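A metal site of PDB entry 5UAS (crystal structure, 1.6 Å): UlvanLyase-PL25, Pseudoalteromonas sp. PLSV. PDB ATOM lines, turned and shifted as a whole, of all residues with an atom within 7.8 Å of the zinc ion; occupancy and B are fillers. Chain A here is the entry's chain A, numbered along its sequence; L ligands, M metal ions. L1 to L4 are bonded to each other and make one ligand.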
ATOM      1  N   ASN A 132     -19.683  24.157 -14.494  1.00  0.00           N
ATOM      2  CA  ASN A 132     -19.016  22.862 -14.467  1.00  0.00           C
ATOM      3  C   ASN A 132     -18.579  22.513 -15.885  1.00  0.00           C
ATOM      4  O   ASN A 132     -18.735  23.309 -16.811  1.00  0.00           O
ATOM      5  CB  ASN A 132     -19.940  21.783 -13.854  1.00  0.00           C
ATOM      6  CG  ASN A 132     -21.131  21.419 -14.775  1.00  0.00           C
ATOM      7  OD1 ASN A 132     -21.591  22.218 -15.592  1.00  0.00           O
ATOM      8  ND2 ASN A 132     -21.650  20.194 -14.605  1.00  0.00           N
ATOM      9  N   ARG A 180     -23.707  28.732 -23.136  1.00  0.00           N
ATOM     10  CA  ARG A 180     -23.623  28.275 -21.750  1.00  0.00           C
ATOM     11  C   ARG A 180     -22.161  28.045 -21.376  1.00  0.00           C
ATOM     12  O   ARG A 180     -21.445  27.315 -22.080  1.00  0.00           O
ATOM     13  CB  ARG A 180     -24.451  27.012 -21.592  1.00  0.00           C
ATOM     14  CG  ARG A 180     -24.441  26.486 -20.177  1.00  0.00           C
ATOM     15  CD  ARG A 180     -25.203  25.163 -20.143  1.00  0.00           C
ATOM     16  NE  ARG A 180     -24.476  24.113 -20.858  1.00  0.00           N
ATOM     17  CZ  ARG A 180     -24.924  22.889 -21.099  1.00  0.00           C
ATOM     18  NH1 ARG A 180     -26.173  22.536 -20.730  1.00  0.00           N
ATOM     19  NH2 ARG A 180     -24.145  22.015 -21.753  1.00  0.00           N
ATOM     20  N   ALA A 183     -21.005  22.948 -18.718  1.00  0.00           N
ATOM     21  CA  ALA A 183     -22.031  21.921 -18.898  1.00  0.00           C
ATOM     22  C   ALA A 183     -23.298  22.348 -18.148  1.00  0.00           C
ATOM     23  O   ALA A 183     -23.534  23.551 -18.032  1.00  0.00           O
ATOM     24  CB  ALA A 183     -21.506  20.557 -18.448  1.00  0.00           C
ATOM     25  N   HIS A 184     -24.116  21.412 -17.646  1.00  0.00           N
ATOM     26  CA  HIS A 184     -25.433  21.816 -17.135  1.00  0.00           C
ATOM     27  C   HIS A 184     -25.339  22.898 -16.066  1.00  0.00           C
ATOM     28  O   HIS A 184     -26.199  23.793 -15.981  1.00  0.00           O
ATOM     29  CB  HIS A 184     -26.164  20.637 -16.513  1.00  0.00           C
ATOM     30  CG  HIS A 184     -26.709  19.674 -17.496  1.00  0.00           C
ATOM     31  ND1 HIS A 184     -27.743  18.820 -17.187  1.00  0.00           N
ATOM     32  CD2 HIS A 184     -26.347  19.404 -18.767  1.00  0.00           C
ATOM     33  CE1 HIS A 184     -28.024  18.079 -18.254  1.00  0.00           C
ATOM     34  NE2 HIS A 184     -27.173  18.395 -19.213  1.00  0.00           N
ATOM     35  N   ARG A 185     -24.366  22.787 -15.179  1.00  0.00           N
ATOM     36  CA  ARG A 185     -24.418  23.555 -13.940  1.00  0.00           C
ATOM     37  C   ARG A 185     -23.554  24.813 -14.104  1.00  0.00           C
ATOM     38  O   ARG A 185     -22.550  25.013 -13.423  1.00  0.00           O
ATOM     39  CB  ARG A 185     -24.020  22.689 -12.758  1.00  0.00           C
ATOM     40  CG  ARG A 185     -25.103  21.684 -12.429  1.00  0.00           C
ATOM     41  CD  ARG A 185     -24.773  20.736 -11.296  1.00  0.00           C
ATOM     42  NE  ARG A 185     -25.960  19.916 -11.008  1.00  0.00           N
ATOM     43  CZ  ARG A 185     -26.164  19.260  -9.875  1.00  0.00           C
ATOM     44  NH1 ARG A 185     -25.268  19.291  -8.898  1.00  0.00           N
ATOM     45  NH2 ARG A 185     -27.286  18.562  -9.723  1.00  0.00           N
ATOM     46  N   VAL A 218     -29.898  21.937  -8.861  1.00  0.00           N
ATOM     47  CA  VAL A 218     -29.247  23.169  -9.274  1.00  0.00           C
ATOM     48  C   VAL A 218     -30.108  23.830 -10.333  1.00  0.00           C
ATOM     49  O   VAL A 218     -30.586  23.162 -11.255  1.00  0.00           O
ATOM     50  CB  VAL A 218     -27.837  22.883  -9.824  1.00  0.00           C
ATOM     51  CG1 VAL A 218     -27.141  24.153 -10.279  1.00  0.00           C
ATOM     52  CG2 VAL A 218     -27.008  22.119  -8.833  1.00  0.00           C
ATOM     53  N   SER A 220     -30.650  25.528 -13.698  1.00  0.00           N
ATOM     54  CA  SER A 220     -29.992  25.354 -14.994  1.00  0.00           C
ATOM     55  C   SER A 220     -30.923  25.853 -16.085  1.00  0.00           C
ATOM     56  O   SER A 220     -32.136  25.909 -15.913  1.00  0.00           O
ATOM     57  CB  SER A 220     -29.630  23.866 -15.198  1.00  0.00           C
ATOM     58  OG  SER A 220     -28.886  23.639 -16.379  1.00  0.00           O
ATOM     59  N   TYR A 222     -31.654  26.771 -20.571  1.00  0.00           N
ATOM     60  CA  TYR A 222     -31.357  26.684 -21.999  1.00  0.00           C
ATOM     61  C   TYR A 222     -31.964  27.922 -22.663  1.00  0.00           C
ATOM     62  O   TYR A 222     -33.167  28.119 -22.593  1.00  0.00           O
ATOM     63  CB  TYR A 222     -31.909  25.380 -22.617  1.00  0.00           C
ATOM     64  CG  TYR A 222     -31.253  24.129 -22.087  1.00  0.00           C
ATOM     65  CD1 TYR A 222     -31.767  23.459 -20.994  1.00  0.00           C
ATOM     66  CD2 TYR A 222     -30.129  23.580 -22.708  1.00  0.00           C
ATOM     67  CE1 TYR A 222     -31.164  22.292 -20.506  1.00  0.00           C
ATOM     68  CE2 TYR A 222     -29.526  22.414 -22.220  1.00  0.00           C
ATOM     69  CZ  TYR A 222     -30.046  21.788 -21.118  1.00  0.00           C
ATOM     70  OH  TYR A 222     -29.469  20.632 -20.598  1.00  0.00           O
ATOM     71  N   HIS A 240     -34.139  24.186 -16.547  1.00  0.00           N
ATOM     72  CA  HIS A 240     -33.772  22.792 -16.336  1.00  0.00           C
ATOM     73  C   HIS A 240     -33.656  22.556 -14.836  1.00  0.00           C
ATOM     74  O   HIS A 240     -32.849  23.196 -14.145  1.00  0.00           O
ATOM     75  CB  HIS A 240     -32.460  22.475 -17.058  1.00  0.00           C
ATOM     76  CG  HIS A 240     -31.840  21.152 -16.694  1.00  0.00           C
ATOM     77  ND1 HIS A 240     -32.565  19.975 -16.658  1.00  0.00           N
ATOM     78  CD2 HIS A 240     -30.561  20.822 -16.387  1.00  0.00           C
ATOM     79  CE1 HIS A 240     -31.756  18.986 -16.314  1.00  0.00           C
ATOM     80  NE2 HIS A 240     -30.533  19.470 -16.146  1.00  0.00           N
ATOM     81  N   VAL A 241     -34.476  21.635 -14.321  1.00  0.00           N
ATOM     82  CA  VAL A 241     -34.342  21.172 -12.939  1.00  0.00           C
ATOM     83  C   VAL A 241     -33.207  20.162 -12.944  1.00  0.00           C
ATOM     84  O   VAL A 241     -33.395  19.008 -13.353  1.00  0.00           O
ATOM     85  CB  VAL A 241     -35.647  20.566 -12.403  1.00  0.00           C
ATOM     86  CG1 VAL A 241     -35.538  20.351 -10.896  1.00  0.00           C
ATOM     87  CG2 VAL A 241     -36.840  21.448 -12.761  1.00  0.00           C
ATOM     88  N   CYS A 242     -32.022  20.576 -12.512  1.00  0.00           N
ATOM     89  CA  CYS A 242     -30.834  19.729 -12.610  1.00  0.00           C
ATOM     90  C   CYS A 242     -30.670  18.964 -11.305  1.00  0.00           C
ATOM     91  O   CYS A 242     -29.987  19.395 -10.366  1.00  0.00           O
ATOM     92  CB  CYS A 242     -29.609  20.561 -12.956  1.00  0.00           C
ATOM     93  SG  CYS A 242     -28.204  19.552 -13.539  1.00  0.00           S
ATOM     94  N   TRP A 243     -31.298  17.788 -11.247  1.00  0.00           N
ATOM     95  CA  TRP A 243     -31.361  17.005 -10.015  1.00  0.00           C
ATOM     96  C   TRP A 243     -30.003  16.406  -9.680  1.00  0.00           C
ATOM     97  O   TRP A 243     -29.281  15.909 -10.549  1.00  0.00           O
ATOM     98  CB  TRP A 243     -32.388  15.866 -10.142  1.00  0.00           C
ATOM     99  CG  TRP A 243     -33.817  16.291 -10.140  1.00  0.00           C
ATOM    100  CD1 TRP A 243     -34.661  16.359 -11.229  1.00  0.00           C
ATOM    101  CD2 TRP A 243     -34.585  16.705  -9.010  1.00  0.00           C
ATOM    102  NE1 TRP A 243     -35.910  16.791 -10.821  1.00  0.00           N
ATOM    103  CE2 TRP A 243     -35.884  17.010  -9.475  1.00  0.00           C
ATOM    104  CE3 TRP A 243     -34.310  16.845  -7.642  1.00  0.00           C
ATOM    105  CZ2 TRP A 243     -36.904  17.434  -8.608  1.00  0.00           C
ATOM    106  CZ3 TRP A 243     -35.333  17.283  -6.792  1.00  0.00           C
ATOM    107  CH2 TRP A 243     -36.601  17.573  -7.282  1.00  0.00           C
ATOM    108  N   ASP A 244     -29.664  16.436  -8.394  1.00  0.00           N
ATOM    109  CA  ASP A 244     -28.525  15.652  -7.925  1.00  0.00           C
ATOM    110  C   ASP A 244     -28.809  14.171  -8.174  1.00  0.00           C
ATOM    111  O   ASP A 244     -29.952  13.734  -8.237  1.00  0.00           O
ATOM    112  CB  ASP A 244     -28.270  15.908  -6.432  1.00  0.00           C
ATOM    113  CG  ASP A 244     -27.903  17.351  -6.131  1.00  0.00           C
ATOM    114  OD1 ASP A 244     -27.654  18.115  -7.094  1.00  0.00           O
ATOM    115  OD2 ASP A 244     -27.887  17.726  -4.936  1.00  0.00           O
ATOM    116  N   HIS A 254     -30.895  12.261 -12.059  1.00  0.00           N
ATOM    117  CA  HIS A 254     -30.721  13.351 -13.009  1.00  0.00           C
ATOM    118  C   HIS A 254     -31.293  12.957 -14.367  1.00  0.00           C
ATOM    119  O   HIS A 254     -30.883  11.951 -14.959  1.00  0.00           O
ATOM    120  CB  HIS A 254     -29.239  13.732 -13.114  1.00  0.00           C
ATOM    121  CG  HIS A 254     -28.985  14.808 -14.117  1.00  0.00           C
ATOM    122  ND1 HIS A 254     -28.654  14.539 -15.422  1.00  0.00           N
ATOM    123  CD2 HIS A 254     -29.059  16.157 -14.020  1.00  0.00           C
ATOM    124  CE1 HIS A 254     -28.502  15.678 -16.078  1.00  0.00           C
ATOM    125  NE2 HIS A 254     -28.734  16.677 -15.246  1.00  0.00           N
ATOM    126  N   THR A 255     -32.222  13.752 -14.848  1.00  0.00           N
ATOM    127  CA  THR A 255     -32.884  13.582 -16.135  1.00  0.00           C
ATOM    128  C   THR A 255     -32.661  14.846 -16.961  1.00  0.00           C
ATOM    129  O   THR A 255     -31.892  15.740 -16.570  1.00  0.00           O
ATOM    130  CB  THR A 255     -34.372  13.363 -15.927  1.00  0.00           C
ATOM    131  OG1 THR A 255     -34.901  14.531 -15.287  1.00  0.00           O
ATOM    132  CG2 THR A 255     -34.618  12.142 -15.031  1.00  0.00           C
ATOM    133  N   THR A 256     -33.351  14.945 -18.104  1.00  0.00           N
ATOM    134  CA  THR A 256     -33.396  16.184 -18.876  1.00  0.00           C
ATOM    135  C   THR A 256     -34.604  17.058 -18.502  1.00  0.00           C
ATOM    136  O   THR A 256     -34.991  17.925 -19.300  1.00  0.00           O
ATOM    137  CB  THR A 256     -33.413  15.907 -20.385  1.00  0.00           C
ATOM    138  OG1 THR A 256     -34.629  15.247 -20.762  1.00  0.00           O
ATOM    139  CG2 THR A 256     -32.200  15.045 -20.786  1.00  0.00           C
ATOM    140  N   GLU A 257     -35.203  16.851 -17.327  1.00  0.00           N
ATOM    141  CA  GLU A 257     -36.413  17.596 -16.942  1.00  0.00           C
ATOM    142  C   GLU A 257     -36.229  19.096 -17.153  1.00  0.00           C
ATOM    143  O   GLU A 257     -35.334  19.718 -16.574  1.00  0.00           O
ATOM    144  CB  GLU A 257     -36.782  17.297 -15.486  1.00  0.00           C
ATOM    145  CG  GLU A 257     -37.976  18.113 -14.998  1.00  0.00           C
ATOM    146  CD  GLU A 257     -38.491  17.709 -13.616  1.00  0.00           C
ATOM    147  OE1 GLU A 257     -37.902  16.795 -12.977  1.00  0.00           O
ATOM    148  OE2 GLU A 257     -39.491  18.299 -13.171  1.00  0.00           O
HETATM  149  C1  LIG L   1     -23.777  14.876 -17.765  1.00  0.00           C
HETATM  150  C2  LIG L   1     -24.711  13.927 -18.505  1.00  0.00           C
HETATM  151  C3  LIG L   1     -25.750  14.701 -19.294  1.00  0.00           C
HETATM  152  C4  LIG L   1     -25.048  15.632 -20.291  1.00  0.00           C
HETATM  153  C5  LIG L   1     -24.153  16.560 -19.453  1.00  0.00           C
HETATM  154  C6  LIG L   1     -23.378  17.558 -20.291  1.00  0.00           C
HETATM  155  O1  LIG L   1     -24.522  15.581 -16.756  1.00  0.00           O
HETATM  156  O2  LIG L   1     -28.945  12.957 -20.341  1.00  0.00           O
HETATM  157  O3  LIG L   1     -23.958  13.090 -19.389  1.00  0.00           O
HETATM  158  O4  LIG L   1     -28.198  13.199 -18.053  1.00  0.00           O
HETATM  159  O5  LIG L   1     -26.669  13.814 -19.920  1.00  0.00           O
HETATM  160  O6  LIG L   1     -28.693  15.151 -19.372  1.00  0.00           O
HETATM  161  O7  LIG L   1     -23.200  15.798 -18.700  1.00  0.00           O
HETATM  162  S1  LIG L   1     -28.129  13.780 -19.403  1.00  0.00           S
HETATM  163  O8  LIG L   1     -26.025  16.382 -21.031  1.00  0.00           O
HETATM  164  C1  LG2 L   2     -26.208  15.987 -22.402  1.00  0.00           C
HETATM  165  C2  LG2 L   2     -27.659  15.507 -22.624  1.00  0.00           C
HETATM  166  C3  LG2 L   2     -28.530  16.713 -22.488  1.00  0.00           C
HETATM  167  C4  LG2 L   2     -28.141  17.801 -23.433  1.00  0.00           C
HETATM  168  C5  LG2 L   2     -26.721  18.155 -23.251  1.00  0.00           C
HETATM  169  C6  LG2 L   2     -26.359  19.279 -22.223  1.00  0.00           C
HETATM  170  O1  LG2 L   2     -27.761  14.891 -23.915  1.00  0.00           O
HETATM  171  O2  LG2 L   2     -28.665  17.160 -21.129  1.00  0.00           O
HETATM  172  O3  LG2 L   2     -28.503  17.713 -24.822  1.00  0.00           O
HETATM  173  O4  LG2 L   2     -25.816  17.100 -23.268  1.00  0.00           O
HETATM  174  O5  LG2 L   2     -27.212  20.071 -21.817  1.00  0.00           O
HETATM  175  O6  LG2 L   2     -25.187  19.386 -21.835  1.00  0.00           O
HETATM  176  C1  LG3 L   3     -29.598  18.495 -25.302  1.00  0.00           C
HETATM  177  C2  LG3 L   3     -29.378  18.608 -26.801  1.00  0.00           C
HETATM  178  C3  LG3 L   3     -29.438  17.229 -27.475  1.00  0.00           C
HETATM  179  C4  LG3 L   3     -30.693  16.437 -27.101  1.00  0.00           C
HETATM  180  C5  LG3 L   3     -30.884  16.465 -25.596  1.00  0.00           C
HETATM  181  C6  LG3 L   3     -32.247  15.865 -25.240  1.00  0.00           C
HETATM  182  O1  LG3 L   3     -28.318  17.703 -31.043  1.00  0.00           O
HETATM  183  O2  LG3 L   3     -30.357  19.465 -27.343  1.00  0.00           O
HETATM  184  O3  LG3 L   3     -27.957  15.627 -29.699  1.00  0.00           O
HETATM  185  O4  LG3 L   3     -29.385  17.430 -28.875  1.00  0.00           O
HETATM  186  O5  LG3 L   3     -26.967  17.748 -29.074  1.00  0.00           O
HETATM  187  O6  LG3 L   3     -30.788  17.777 -25.040  1.00  0.00           O
HETATM  188  S1  LG3 L   3     -28.113  17.095 -29.716  1.00  0.00           S
HETATM  189  O7  LG3 L   3     -30.549  15.055 -27.478  1.00  0.00           O
HETATM  190  C1  LG4 L   4     -31.215  14.755 -28.706  1.00  0.00           C
HETATM  191  C2  LG4 L   4     -30.670  13.428 -29.236  1.00  0.00           C
HETATM  192  C3  LG4 L   4     -30.883  12.356 -28.173  1.00  0.00           C
HETATM  193  C4  LG4 L   4     -32.289  12.398 -27.646  1.00  0.00           C
HETATM  194  C5  LG4 L   4     -33.080  13.473 -27.797  1.00  0.00           C
HETATM  195  C6  LG4 L   4     -34.456  13.435 -27.313  1.00  0.00           C
HETATM  196  O1  LG4 L   4     -31.324  13.078 -30.468  1.00  0.00           O
HETATM  197  O2  LG4 L   4     -29.992  12.502 -27.069  1.00  0.00           O
HETATM  198  O3  LG4 L   4     -32.619  14.666 -28.473  1.00  0.00           O
HETATM  199  O4  LG4 L   4     -34.902  12.370 -26.816  1.00  0.00           O
HETATM  200  O5  LG4 L   4     -35.170  14.446 -27.428  1.00  0.00           O
HETATM  201 ZN    ZN M   1     -28.811  18.599 -15.448  1.00  0.00          ZN
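An oxygen (O6) of LG2 L2 lies within salt-bridge range of the guanidinium group (NH2) of Arg 180 (2.8 Å).
The side-chain hydroxyl (OH) of Tyr 222 sits at hydrogen-bond distance from an oxygen (O5) of LG2 L2, at 2.6 Å.
ND1 of His 254 is in hydrogen-bond range of O4 of LIG L1, 3.0 Å away.
A ring nitrogen (NE2) of His 184 sits at hydrogen-bond distance from an oxygen (O2) of LG2 L2.
The nearest printed residue that does not touch the zinc ion is Thr 255 (4.4 Å).
N of His 184 lies within hydrogen-bond range of OD1 of Asn 132, 3.4 Å away.
The backbone carbonyl oxygen of Cys 242 lies within hydrogen-bond range of the guanidinium group of Arg 185, 2.9 Å away.
O of Glu 257 lies within hydrogen-bond range of ND1 of His 240.
The backbone carbonyl oxygen of Cys 242 sits at hydrogen-bond distance from the backbone NH of Val 218 (3.0 Å).
The backbone NH of His 240 is in hydrogen-bond range of the backbone carbonyl oxygen of Ser 220 (2.7 Å).
OG of Ser 220 lies within hydrogen-bond range of O of His 184 (2.7 Å).
NE2 of His 184 lies within hydrogen-bond range of OH of Tyr 222, 3.5 Å away.
The zinc ion is bound by a ring nitrogen (NE2) of His 254, a ring nitrogen (NE2) of His 240, a ring nitrogen (ND1) of His 184 and the side-chain sulfur of Cys 242.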
